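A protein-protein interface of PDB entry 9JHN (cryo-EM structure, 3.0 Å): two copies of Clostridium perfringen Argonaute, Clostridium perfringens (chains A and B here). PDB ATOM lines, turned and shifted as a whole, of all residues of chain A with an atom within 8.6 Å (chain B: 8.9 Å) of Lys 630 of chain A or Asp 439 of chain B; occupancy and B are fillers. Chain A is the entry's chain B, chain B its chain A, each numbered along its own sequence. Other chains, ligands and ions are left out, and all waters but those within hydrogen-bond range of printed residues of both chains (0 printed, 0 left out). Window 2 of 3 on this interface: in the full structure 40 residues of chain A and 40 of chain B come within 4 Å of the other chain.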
ATOM      1  N   GLN A 588      -9.570 -31.944  28.013  1.00  0.00           N
ATOM      2  CA  GLN A 588      -9.130 -30.573  28.250  1.00  0.00           C
ATOM      3  C   GLN A 588      -7.826 -30.290  27.518  1.00  0.00           C
ATOM      4  O   GLN A 588      -7.731 -29.313  26.772  1.00  0.00           O
ATOM      5  CB  GLN A 588      -8.966 -30.337  29.750  1.00  0.00           C
ATOM      6  CG  GLN A 588      -8.746 -28.899  30.174  1.00  0.00           C
ATOM      7  CD  GLN A 588      -9.982 -28.055  29.986  1.00  0.00           C
ATOM      8  OE1 GLN A 588     -10.043 -27.221  29.096  1.00  0.00           O
ATOM      9  NE2 GLN A 588     -10.986 -28.283  30.821  1.00  0.00           N
ATOM     10  N   ASP A 592      -8.066 -27.942  24.190  1.00  0.00           N
ATOM     11  CA  ASP A 592      -7.324 -26.698  24.311  1.00  0.00           C
ATOM     12  C   ASP A 592      -6.221 -26.622  23.275  1.00  0.00           C
ATOM     13  O   ASP A 592      -5.989 -25.559  22.698  1.00  0.00           O
ATOM     14  CB  ASP A 592      -6.742 -26.561  25.702  1.00  0.00           C
ATOM     15  CG  ASP A 592      -7.783 -26.266  26.738  1.00  0.00           C
ATOM     16  OD1 ASP A 592      -8.845 -25.718  26.387  1.00  0.00           O
ATOM     17  OD2 ASP A 592      -7.522 -26.573  27.916  1.00  0.00           O
ATOM     18  N   LEU A 595      -8.001 -25.692  19.921  1.00  0.00           N
ATOM     19  CA  LEU A 595      -8.399 -24.295  19.793  1.00  0.00           C
ATOM     20  C   LEU A 595      -7.185 -23.381  19.751  1.00  0.00           C
ATOM     21  O   LEU A 595      -7.186 -22.379  19.033  1.00  0.00           O
ATOM     22  CB  LEU A 595      -9.323 -23.918  20.944  1.00  0.00           C
ATOM     23  CG  LEU A 595     -10.565 -24.800  20.967  1.00  0.00           C
ATOM     24  CD1 LEU A 595     -11.424 -24.527  22.154  1.00  0.00           C
ATOM     25  CD2 LEU A 595     -11.353 -24.672  19.717  1.00  0.00           C
ATOM     26  N   TYR A 605     -11.098 -18.396  17.053  1.00  0.00           N
ATOM     27  CA  TYR A 605     -11.632 -19.705  17.380  1.00  0.00           C
ATOM     28  C   TYR A 605     -12.480 -20.233  16.223  1.00  0.00           C
ATOM     29  O   TYR A 605     -13.010 -19.454  15.428  1.00  0.00           O
ATOM     30  CB  TYR A 605     -12.466 -19.646  18.658  1.00  0.00           C
ATOM     31  CG  TYR A 605     -11.658 -19.708  19.926  1.00  0.00           C
ATOM     32  CD1 TYR A 605     -10.315 -20.065  19.899  1.00  0.00           C
ATOM     33  CD2 TYR A 605     -12.242 -19.447  21.155  1.00  0.00           C
ATOM     34  CE1 TYR A 605      -9.576 -20.133  21.052  1.00  0.00           C
ATOM     35  CE2 TYR A 605     -11.507 -19.515  22.317  1.00  0.00           C
ATOM     36  CZ  TYR A 605     -10.175 -19.858  22.257  1.00  0.00           C
ATOM     37  OH  TYR A 605      -9.445 -19.927  23.413  1.00  0.00           O
ATOM     38  N   TRP A 623     -19.491 -32.835  29.236  1.00  0.00           N
ATOM     39  CA  TRP A 623     -18.213 -32.130  29.176  1.00  0.00           C
ATOM     40  C   TRP A 623     -18.087 -31.337  27.891  1.00  0.00           C
ATOM     41  O   TRP A 623     -17.599 -30.205  27.905  1.00  0.00           O
ATOM     42  CB  TRP A 623     -17.031 -33.090  29.255  1.00  0.00           C
ATOM     43  CG  TRP A 623     -15.726 -32.346  29.371  1.00  0.00           C
ATOM     44  CD1 TRP A 623     -15.162 -31.872  30.512  1.00  0.00           C
ATOM     45  CD2 TRP A 623     -14.898 -31.874  28.295  1.00  0.00           C
ATOM     46  NE1 TRP A 623     -14.001 -31.205  30.227  1.00  0.00           N
ATOM     47  CE2 TRP A 623     -13.826 -31.177  28.871  1.00  0.00           C
ATOM     48  CE3 TRP A 623     -14.956 -31.990  26.902  1.00  0.00           C
ATOM     49  CZ2 TRP A 623     -12.816 -30.608  28.108  1.00  0.00           C
ATOM     50  CZ3 TRP A 623     -13.961 -31.418  26.152  1.00  0.00           C
ATOM     51  CH2 TRP A 623     -12.904 -30.737  26.754  1.00  0.00           C
ATOM     52  N   TYR A 624     -18.463 -31.940  26.763  1.00  0.00           N
ATOM     53  CA  TYR A 624     -18.371 -31.254  25.480  1.00  0.00           C
ATOM     54  C   TYR A 624     -19.312 -30.062  25.421  1.00  0.00           C
ATOM     55  O   TYR A 624     -18.933 -28.987  24.949  1.00  0.00           O
ATOM     56  CB  TYR A 624     -18.672 -32.215  24.333  1.00  0.00           C
ATOM     57  CG  TYR A 624     -17.598 -33.224  24.031  1.00  0.00           C
ATOM     58  CD1 TYR A 624     -16.477 -32.873  23.303  1.00  0.00           C
ATOM     59  CD2 TYR A 624     -17.721 -34.535  24.448  1.00  0.00           C
ATOM     60  CE1 TYR A 624     -15.499 -33.800  23.021  1.00  0.00           C
ATOM     61  CE2 TYR A 624     -16.751 -35.463  24.174  1.00  0.00           C
ATOM     62  CZ  TYR A 624     -15.646 -35.092  23.462  1.00  0.00           C
ATOM     63  OH  TYR A 624     -14.689 -36.033  23.188  1.00  0.00           O
ATOM     64  N   GLU A 625     -20.541 -30.229  25.915  1.00  0.00           N
ATOM     65  CA  GLU A 625     -21.495 -29.127  25.888  1.00  0.00           C
ATOM     66  C   GLU A 625     -21.052 -27.995  26.801  1.00  0.00           C
ATOM     67  O   GLU A 625     -21.162 -26.824  26.431  1.00  0.00           O
ATOM     68  CB  GLU A 625     -22.890 -29.615  26.265  1.00  0.00           C
ATOM     69  CG  GLU A 625     -23.528 -30.504  25.222  1.00  0.00           C
ATOM     70  CD  GLU A 625     -24.916 -30.945  25.613  1.00  0.00           C
ATOM     71  OE1 GLU A 625     -25.353 -30.618  26.733  1.00  0.00           O
ATOM     72  OE2 GLU A 625     -25.570 -31.629  24.803  1.00  0.00           O
ATOM     73  N   ASN A 626     -20.465 -28.329  27.956  1.00  0.00           N
ATOM     74  CA  ASN A 626     -19.911 -27.311  28.845  1.00  0.00           C
ATOM     75  C   ASN A 626     -18.737 -26.589  28.192  1.00  0.00           C
ATOM     76  O   ASN A 626     -18.724 -25.355  28.112  1.00  0.00           O
ATOM     77  CB  ASN A 626     -19.476 -27.970  30.154  1.00  0.00           C
ATOM     78  CG  ASN A 626     -19.152 -26.972  31.248  1.00  0.00           C
ATOM     79  OD1 ASN A 626     -19.286 -25.761  31.077  1.00  0.00           O
ATOM     80  ND2 ASN A 626     -18.713 -27.486  32.390  1.00  0.00           N
ATOM     81  N   TYR A 627     -17.763 -27.352  27.686  1.00  0.00           N
ATOM     82  CA  TYR A 627     -16.518 -26.788  27.178  1.00  0.00           C
ATOM     83  C   TYR A 627     -16.735 -25.965  25.921  1.00  0.00           C
ATOM     84  O   TYR A 627     -16.005 -25.001  25.676  1.00  0.00           O
ATOM     85  CB  TYR A 627     -15.528 -27.912  26.895  1.00  0.00           C
ATOM     86  CG  TYR A 627     -14.196 -27.454  26.369  1.00  0.00           C
ATOM     87  CD1 TYR A 627     -13.223 -26.984  27.222  1.00  0.00           C
ATOM     88  CD2 TYR A 627     -13.915 -27.493  25.013  1.00  0.00           C
ATOM     89  CE1 TYR A 627     -12.007 -26.572  26.742  1.00  0.00           C
ATOM     90  CE2 TYR A 627     -12.710 -27.071  24.527  1.00  0.00           C
ATOM     91  CZ  TYR A 627     -11.760 -26.616  25.397  1.00  0.00           C
ATOM     92  OH  TYR A 627     -10.549 -26.200  24.919  1.00  0.00           O
ATOM     93  N   PHE A 628     -17.709 -26.331  25.100  1.00  0.00           N
ATOM     94  CA  PHE A 628     -17.930 -25.586  23.876  1.00  0.00           C
ATOM     95  C   PHE A 628     -19.131 -24.661  23.950  1.00  0.00           C
ATOM     96  O   PHE A 628     -19.397 -23.949  22.979  1.00  0.00           O
ATOM     97  CB  PHE A 628     -18.083 -26.540  22.697  1.00  0.00           C
ATOM     98  CG  PHE A 628     -16.848 -27.331  22.397  1.00  0.00           C
ATOM     99  CD1 PHE A 628     -15.764 -26.735  21.796  1.00  0.00           C
ATOM    100  CD2 PHE A 628     -16.786 -28.678  22.686  1.00  0.00           C
ATOM    101  CE1 PHE A 628     -14.633 -27.462  21.527  1.00  0.00           C
ATOM    102  CE2 PHE A 628     -15.658 -29.407  22.412  1.00  0.00           C
ATOM    103  CZ  PHE A 628     -14.586 -28.798  21.830  1.00  0.00           C
ATOM    104  N   GLY A 629     -19.861 -24.641  25.063  1.00  0.00           N
ATOM    105  CA  GLY A 629     -20.871 -23.623  25.246  1.00  0.00           C
ATOM    106  C   GLY A 629     -20.282 -22.493  26.051  1.00  0.00           C
ATOM    107  O   GLY A 629     -20.797 -21.372  26.053  1.00  0.00           O
ATOM    108  N   LYS A 630     -19.180 -22.790  26.738  1.00  0.00           N
ATOM    109  CA  LYS A 630     -18.432 -21.742  27.411  1.00  0.00           C
ATOM    110  C   LYS A 630     -17.689 -20.870  26.406  1.00  0.00           C
ATOM    111  O   LYS A 630     -17.386 -19.707  26.696  1.00  0.00           O
ATOM    112  CB  LYS A 630     -17.473 -22.387  28.412  1.00  0.00           C
ATOM    113  CG  LYS A 630     -16.761 -21.446  29.348  1.00  0.00           C
ATOM    114  CD  LYS A 630     -15.947 -22.225  30.347  1.00  0.00           C
ATOM    115  CE  LYS A 630     -14.754 -22.852  29.666  1.00  0.00           C
ATOM    116  NZ  LYS A 630     -13.800 -21.807  29.202  1.00  0.00           N
ATOM    117  N   LYS A 631     -17.423 -21.396  25.211  1.00  0.00           N
ATOM    118  CA  LYS A 631     -16.651 -20.695  24.196  1.00  0.00           C
ATOM    119  C   LYS A 631     -17.453 -20.387  22.945  1.00  0.00           C
ATOM    120  O   LYS A 631     -16.872 -19.897  21.971  1.00  0.00           O
ATOM    121  CB  LYS A 631     -15.428 -21.515  23.818  1.00  0.00           C
ATOM    122  CG  LYS A 631     -14.517 -21.750  24.966  1.00  0.00           C
ATOM    123  CD  LYS A 631     -13.387 -22.599  24.537  1.00  0.00           C
ATOM    124  CE  LYS A 631     -12.486 -22.836  25.685  1.00  0.00           C
ATOM    125  NZ  LYS A 631     -13.245 -23.559  26.716  1.00  0.00           N
ATOM    126  N   ASN A 632     -18.758 -20.686  22.950  1.00  0.00           N
ATOM    127  CA  ASN A 632     -19.690 -20.410  21.849  1.00  0.00           C
ATOM    128  C   ASN A 632     -19.255 -21.105  20.560  1.00  0.00           C
ATOM    129  O   ASN A 632     -19.276 -20.527  19.474  1.00  0.00           O
ATOM    130  CB  ASN A 632     -19.868 -18.907  21.633  1.00  0.00           C
ATOM    131  CG  ASN A 632     -20.474 -18.221  22.832  1.00  0.00           C
ATOM    132  OD1 ASN A 632     -21.394 -18.742  23.460  1.00  0.00           O
ATOM    133  ND2 ASN A 632     -19.951 -17.048  23.167  1.00  0.00           N
ATOM    134  N   ILE A 633     -18.852 -22.363  20.698  1.00  0.00           N
ATOM    135  CA  ILE A 633     -18.403 -23.190  19.586  1.00  0.00           C
ATOM    136  C   ILE A 633     -19.455 -24.260  19.350  1.00  0.00           C
ATOM    137  O   ILE A 633     -19.714 -25.083  20.235  1.00  0.00           O
ATOM    138  CB  ILE A 633     -17.042 -23.835  19.874  1.00  0.00           C
ATOM    139  CG1 ILE A 633     -15.966 -22.778  20.047  1.00  0.00           C
ATOM    140  CG2 ILE A 633     -16.653 -24.754  18.764  1.00  0.00           C
ATOM    141  CD1 ILE A 633     -14.698 -23.337  20.585  1.00  0.00           C
ATOM    142  N   PHE A 635     -20.356 -27.739  17.890  1.00  0.00           N
ATOM    143  CA  PHE A 635     -19.517 -28.905  17.677  1.00  0.00           C
ATOM    144  C   PHE A 635     -20.378 -30.079  17.245  1.00  0.00           C
ATOM    145  O   PHE A 635     -21.597 -30.079  17.411  1.00  0.00           O
ATOM    146  CB  PHE A 635     -18.708 -29.263  18.926  1.00  0.00           C
ATOM    147  CG  PHE A 635     -19.537 -29.742  20.063  1.00  0.00           C
ATOM    148  CD1 PHE A 635     -20.162 -28.843  20.904  1.00  0.00           C
ATOM    149  CD2 PHE A 635     -19.652 -31.089  20.327  1.00  0.00           C
ATOM    150  CE1 PHE A 635     -20.920 -29.276  21.952  1.00  0.00           C
ATOM    151  CE2 PHE A 635     -20.411 -31.527  21.368  1.00  0.00           C
ATOM    152  CZ  PHE A 635     -21.041 -30.621  22.187  1.00  0.00           C
ATOM    153  N   TYR B 435      -1.460 -12.616  33.944  1.00  0.00           N
ATOM    154  CA  TYR B 435      -2.548 -13.458  33.472  1.00  0.00           C
ATOM    155  C   TYR B 435      -3.702 -13.438  34.460  1.00  0.00           C
ATOM    156  O   TYR B 435      -3.488 -13.511  35.673  1.00  0.00           O
ATOM    157  CB  TYR B 435      -2.074 -14.892  33.224  1.00  0.00           C
ATOM    158  CG  TYR B 435      -1.630 -15.689  34.427  1.00  0.00           C
ATOM    159  CD1 TYR B 435      -0.331 -15.622  34.882  1.00  0.00           C
ATOM    160  CD2 TYR B 435      -2.497 -16.562  35.060  1.00  0.00           C
ATOM    161  CE1 TYR B 435       0.081 -16.369  35.959  1.00  0.00           C
ATOM    162  CE2 TYR B 435      -2.092 -17.310  36.134  1.00  0.00           C
ATOM    163  CZ  TYR B 435      -0.802 -17.211  36.577  1.00  0.00           C
ATOM    164  OH  TYR B 435      -0.391 -17.958  37.648  1.00  0.00           O
ATOM    165  N   GLU B 436      -4.918 -13.335  33.932  1.00  0.00           N
ATOM    166  CA  GLU B 436      -6.112 -13.387  34.760  1.00  0.00           C
ATOM    167  C   GLU B 436      -6.322 -14.803  35.268  1.00  0.00           C
ATOM    168  O   GLU B 436      -6.202 -15.766  34.507  1.00  0.00           O
ATOM    169  CB  GLU B 436      -7.332 -12.944  33.958  1.00  0.00           C
ATOM    170  CG  GLU B 436      -7.337 -11.488  33.527  1.00  0.00           C
ATOM    171  CD  GLU B 436      -7.545 -10.532  34.681  1.00  0.00           C
ATOM    172  OE1 GLU B 436      -8.228 -10.914  35.653  1.00  0.00           O
ATOM    173  OE2 GLU B 436      -7.041  -9.392  34.608  1.00  0.00           O
ATOM    174  N   LEU B 437      -6.631 -14.932  36.552  1.00  0.00           N
ATOM    175  CA  LEU B 437      -7.009 -16.228  37.092  1.00  0.00           C
ATOM    176  C   LEU B 437      -8.383 -16.611  36.568  1.00  0.00           C
ATOM    177  O   LEU B 437      -9.271 -15.766  36.438  1.00  0.00           O
ATOM    178  CB  LEU B 437      -7.014 -16.189  38.614  1.00  0.00           C
ATOM    179  CG  LEU B 437      -5.662 -15.880  39.249  1.00  0.00           C
ATOM    180  CD1 LEU B 437      -5.818 -15.713  40.742  1.00  0.00           C
ATOM    181  CD2 LEU B 437      -4.670 -16.967  38.932  1.00  0.00           C
ATOM    182  N   GLY B 438      -8.562 -17.890  36.262  1.00  0.00           N
ATOM    183  CA  GLY B 438      -9.741 -18.283  35.521  1.00  0.00           C
ATOM    184  C   GLY B 438      -9.607 -19.612  34.816  1.00  0.00           C
ATOM    185  O   GLY B 438      -9.308 -20.631  35.445  1.00  0.00           O
ATOM    186  N   ASP B 439      -9.855 -19.613  33.510  1.00  0.00           N
ATOM    187  CA  ASP B 439      -9.911 -20.846  32.743  1.00  0.00           C
ATOM    188  C   ASP B 439      -8.528 -21.453  32.563  1.00  0.00           C
ATOM    189  O   ASP B 439      -7.502 -20.819  32.810  1.00  0.00           O
ATOM    190  CB  ASP B 439     -10.535 -20.588  31.373  1.00  0.00           C
ATOM    191  CG  ASP B 439     -12.003 -20.245  31.460  1.00  0.00           C
ATOM    192  OD1 ASP B 439     -12.679 -20.728  32.393  1.00  0.00           O
ATOM    193  OD2 ASP B 439     -12.480 -19.487  30.594  1.00  0.00           O
ATOM    194  N   ILE B 440      -8.518 -22.710  32.128  1.00  0.00           N
ATOM    195  CA  ILE B 440      -7.269 -23.407  31.845  1.00  0.00           C
ATOM    196  C   ILE B 440      -6.750 -23.030  30.461  1.00  0.00           C
ATOM    197  O   ILE B 440      -5.538 -22.866  30.256  1.00  0.00           O
ATOM    198  CB  ILE B 440      -7.493 -24.922  32.024  1.00  0.00           C
ATOM    199  CG1 ILE B 440      -7.571 -25.260  33.511  1.00  0.00           C
ATOM    200  CG2 ILE B 440      -6.457 -25.763  31.324  1.00  0.00           C
ATOM    201  CD1 ILE B 440      -7.976 -26.674  33.792  1.00  0.00           C
ATOM    202  N   THR B 441      -7.659 -22.821  29.507  1.00  0.00           N
ATOM    203  CA  THR B 441      -7.250 -22.374  28.181  1.00  0.00           C
ATOM    204  C   THR B 441      -6.680 -20.959  28.205  1.00  0.00           C
ATOM    205  O   THR B 441      -5.817 -20.631  27.386  1.00  0.00           O
ATOM    206  CB  THR B 441      -8.427 -22.475  27.209  1.00  0.00           C
ATOM    207  OG1 THR B 441      -8.018 -22.042  25.907  1.00  0.00           O
ATOM    208  CG2 THR B 441      -9.609 -21.654  27.680  1.00  0.00           C
ATOM    209  N   GLU B 442      -7.082 -20.133  29.172  1.00  0.00           N
ATOM    210  CA  GLU B 442      -6.487 -18.807  29.283  1.00  0.00           C
ATOM    211  C   GLU B 442      -5.090 -18.882  29.878  1.00  0.00           C
ATOM    212  O   GLU B 442      -4.223 -18.078  29.529  1.00  0.00           O
ATOM    213  CB  GLU B 442      -7.382 -17.895  30.113  1.00  0.00           C
ATOM    214  CG  GLU B 442      -8.714 -17.591  29.453  1.00  0.00           C
ATOM    215  CD  GLU B 442      -8.567 -16.764  28.193  1.00  0.00           C
ATOM    216  OE1 GLU B 442      -7.644 -15.926  28.124  1.00  0.00           O
ATOM    217  OE2 GLU B 442      -9.379 -16.955  27.266  1.00  0.00           O
ATOM    218  N   TYR B 443      -4.847 -19.858  30.756  1.00  0.00           N
ATOM    219  CA  TYR B 443      -3.499 -20.095  31.266  1.00  0.00           C
ATOM    220  C   TYR B 443      -2.586 -20.578  30.156  1.00  0.00           C
ATOM    221  O   TYR B 443      -1.420 -20.170  30.062  1.00  0.00           O
ATOM    222  CB  TYR B 443      -3.544 -21.129  32.381  1.00  0.00           C
ATOM    223  CG  TYR B 443      -4.279 -20.684  33.612  1.00  0.00           C
ATOM    224  CD1 TYR B 443      -4.444 -19.340  33.904  1.00  0.00           C
ATOM    225  CD2 TYR B 443      -4.847 -21.610  34.463  1.00  0.00           C
ATOM    226  CE1 TYR B 443      -5.124 -18.938  35.024  1.00  0.00           C
ATOM    227  CE2 TYR B 443      -5.528 -21.217  35.586  1.00  0.00           C
ATOM    228  CZ  TYR B 443      -5.664 -19.882  35.860  1.00  0.00           C
ATOM    229  OH  TYR B 443      -6.350 -19.493  36.983  1.00  0.00           O
ATOM    230  N   LYS B 444      -3.119 -21.427  29.280  1.00  0.00           N
ATOM    231  CA  LYS B 444      -2.337 -21.911  28.152  1.00  0.00           C
ATOM    232  C   LYS B 444      -2.048 -20.796  27.157  1.00  0.00           C
ATOM    233  O   LYS B 444      -0.929 -20.693  26.645  1.00  0.00           O
ATOM    234  CB  LYS B 444      -3.074 -23.061  27.480  1.00  0.00           C
ATOM    235  CG  LYS B 444      -3.177 -24.305  28.330  1.00  0.00           C
ATOM    236  CD  LYS B 444      -3.890 -25.386  27.574  1.00  0.00           C
ATOM    237  CE  LYS B 444      -4.168 -26.598  28.435  1.00  0.00           C
ATOM    238  NZ  LYS B 444      -2.924 -27.316  28.761  1.00  0.00           N
ATOM    239  N   LYS B 445      -3.024 -19.926  26.904  1.00  0.00           N
ATOM    240  CA  LYS B 445      -2.763 -18.803  26.012  1.00  0.00           C
ATOM    241  C   LYS B 445      -1.838 -17.773  26.648  1.00  0.00           C
ATOM    242  O   LYS B 445      -1.101 -17.094  25.933  1.00  0.00           O
ATOM    243  CB  LYS B 445      -4.065 -18.152  25.569  1.00  0.00           C
ATOM    244  CG  LYS B 445      -4.867 -18.997  24.611  1.00  0.00           C
ATOM    245  CD  LYS B 445      -6.021 -18.206  24.054  1.00  0.00           C
ATOM    246  CE  LYS B 445      -7.067 -17.995  25.120  1.00  0.00           C
ATOM    247  NZ  LYS B 445      -8.254 -17.274  24.600  1.00  0.00           N
ATOM    248  N   ALA B 446      -1.830 -17.664  27.980  1.00  0.00           N
ATOM    249  CA  ALA B 446      -0.845 -16.817  28.650  1.00  0.00           C
ATOM    250  C   ALA B 446       0.564 -17.356  28.470  1.00  0.00           C
ATOM    251  O   ALA B 446       1.507 -16.590  28.218  1.00  0.00           O
ATOM    252  CB  ALA B 446      -1.165 -16.704  30.136  1.00  0.00           C
ATOM    253  N   ILE B 471     -10.601 -21.131  42.215  1.00  0.00           N
ATOM    254  CA  ILE B 471     -10.311 -20.869  40.799  1.00  0.00           C
ATOM    255  C   ILE B 471      -8.950 -21.373  40.323  1.00  0.00           C
ATOM    256  O   ILE B 471      -7.925 -21.109  40.962  1.00  0.00           O
ATOM    257  CB  ILE B 471     -10.449 -19.350  40.553  1.00  0.00           C
ATOM    258  CG1 ILE B 471     -11.876 -18.890  40.859  1.00  0.00           C
ATOM    259  CG2 ILE B 471     -10.093 -18.960  39.135  1.00  0.00           C
ATOM    260  CD1 ILE B 471     -12.039 -17.387  40.871  1.00  0.00           C
ATOM    261  N   GLU B 472      -8.965 -22.047  39.159  1.00  0.00           N
ATOM    262  CA  GLU B 472      -8.066 -23.144  38.790  1.00  0.00           C
ATOM    263  C   GLU B 472      -6.585 -22.834  38.965  1.00  0.00           C
ATOM    264  O   GLU B 472      -6.135 -21.710  38.729  1.00  0.00           O
ATOM    265  CB  GLU B 472      -8.323 -23.525  37.333  1.00  0.00           C
ATOM    266  CG  GLU B 472      -9.726 -24.019  37.042  1.00  0.00           C
ATOM    267  CD  GLU B 472     -10.017 -25.371  37.650  1.00  0.00           C
ATOM    268  OE1 GLU B 472      -9.086 -26.199  37.744  1.00  0.00           O
ATOM    269  OE2 GLU B 472     -11.179 -25.608  38.036  1.00  0.00           O
ATOM    270  N   ASN B 473      -5.832 -23.850  39.382  1.00  0.00           N
ATOM    271  CA  ASN B 473      -4.383 -23.748  39.458  1.00  0.00           C
ATOM    272  C   ASN B 473      -3.809 -23.676  38.050  1.00  0.00           C
ATOM    273  O   ASN B 473      -4.346 -24.277  37.117  1.00  0.00           O
ATOM    274  CB  ASN B 473      -3.813 -24.949  40.210  1.00  0.00           C
ATOM    275  CG  ASN B 473      -2.367 -24.765  40.609  1.00  0.00           C
ATOM    276  OD1 ASN B 473      -1.755 -23.748  40.325  1.00  0.00           O
ATOM    277  ND2 ASN B 473      -1.816 -25.758  41.286  1.00  0.00           N
ATOM    278  N   SER B 474      -2.717 -22.938  37.901  1.00  0.00           N
ATOM    279  CA  SER B 474      -2.117 -22.691  36.602  1.00  0.00           C
ATOM    280  C   SER B 474      -0.810 -23.435  36.391  1.00  0.00           C
ATOM    281  O   SER B 474      -0.228 -23.311  35.308  1.00  0.00           O
ATOM    282  CB  SER B 474      -1.862 -21.203  36.429  1.00  0.00           C
ATOM    283  OG  SER B 474      -0.818 -20.789  37.291  1.00  0.00           O
ATOM    284  N   PRO B 477      -1.337 -26.230  33.384  1.00  0.00           N
ATOM    285  CA  PRO B 477      -1.281 -25.697  32.011  1.00  0.00           C
ATOM    286  C   PRO B 477       0.022 -25.014  31.665  1.00  0.00           C
ATOM    287  O   PRO B 477       0.478 -25.137  30.522  1.00  0.00           O
ATOM    288  CB  PRO B 477      -2.442 -24.703  31.970  1.00  0.00           C
ATOM    289  CG  PRO B 477      -3.308 -25.104  33.007  1.00  0.00           C
ATOM    290  CD  PRO B 477      -2.470 -25.606  34.093  1.00  0.00           C
ATOM    291  N   PHE B 478       0.648 -24.322  32.625  1.00  0.00           N
ATOM    292  CA  PHE B 478       1.929 -23.679  32.353  1.00  0.00           C
ATOM    293  C   PHE B 478       3.003 -24.696  32.015  1.00  0.00           C
ATOM    294  O   PHE B 478       3.666 -24.567  30.990  1.00  0.00           O
ATOM    295  CB  PHE B 478       2.374 -22.829  33.538  1.00  0.00           C
ATOM    296  CG  PHE B 478       1.652 -21.531  33.663  1.00  0.00           C
ATOM    297  CD1 PHE B 478       0.833 -21.078  32.654  1.00  0.00           C
ATOM    298  CD2 PHE B 478       1.822 -20.751  34.782  1.00  0.00           C
ATOM    299  CE1 PHE B 478       0.182 -19.898  32.768  1.00  0.00           C
ATOM    300  CE2 PHE B 478       1.175 -19.565  34.895  1.00  0.00           C
ATOM    301  CZ  PHE B 478       0.348 -19.141  33.881  1.00  0.00           C
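The side-chain amino group (NZ) of Lys 445 of chain B sits at hydrogen-bond distance from the side-chain hydroxyl (OH) of Tyr 605 of chain A (3.1 Å). The side-chain carboxylate (OD2) of Asp 439 of chain B lies within salt-bridge range of the side-chain amino group (NZ) of Lys 630 of chain A, at 3.0 Å.
O of Tyr 627 of chain A lies close to NZ of Lys 631 of chain A (3.3 Å). The side-chain hydroxyl (OH) of Tyr 627 of chain A sits at hydrogen-bond distance from the backbone NH (N) of Asp 592 of chain A (3.1 Å). The side-chain carboxylate (OE2) of Glu 442 of chain B is in salt-bridge range of the side-chain amino group (NZ) of Lys 445 of chain B, at 2.9 Å. The side-chain carboxylate (OD2) of Asp 592 of chain A sits close to the side-chain amide oxygen (OE1) of Gln 588 of chain A (2.9 Å).
Of chain B, only Asp 439 comes within 4 Å of Lys 630 of chain A. Of chain A, only Lys 630 (3.0 Å) comes within 4 Å of Asp 439 of chain B. No residue of chain B comes within 4 Å of Gly 629 of chain A. Of chain B, only Thr 441 (3.7 Å) comes within 4 Å of Lys 631 of chain A. Of the printed residues of chain A, Thr 441 of chain B touches Asp 592 (3.4 Å), Tyr 605 (3.6 Å) and Lys 631 (3.7 Å). Printed residues of chain A within 4 Å of Ile 440 of chain B: Asp 592. Ile 471 of chain B touches none of the printed residues of chain A. Glu 472 of chain B touches none of the printed residues of chain A. The nearest residue of chain A that does not touch Asp 439 of chain B is Lys 631 of chain A (5.7 Å).
Of the 18 printed residues of chain B, 5 touch a printed residue of chain A. Of the 16 printed residues of chain A, 4 touch a printed residue of chain B. Printed residues of chain A that touch a printed residue of chain B: Asp 592, Tyr 605, Lys 630 and Lys 631. Among the printed residues, 7 pairs touch across the chains. Among the printed residues, Asp or Glu carboxylates within 4 Å of a Lys or Arg side-chain nitrogen of the other chain: Lys 630 of chain A with Asp 439 of chain B.
No position is printed for both chains. Of the 7 pairs that touch across the chains among the printed residues, none has its exchanged pair printed and touching as well.
OD2 of Asp 592 of chain A touches CG2 of Ile 440 of chain B (3.7 Å). Asp 592 of chain A touches Thr 441 of chain B (OD1 to CB, 3.4 Å). Asp 592 of chain A touches Lys 444 of chain B. OG1 of Thr 441 of chain B touches OH of Tyr 605 of chain A (3.6 Å). Thr 441 of chain B touches Lys 631 of chain A.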
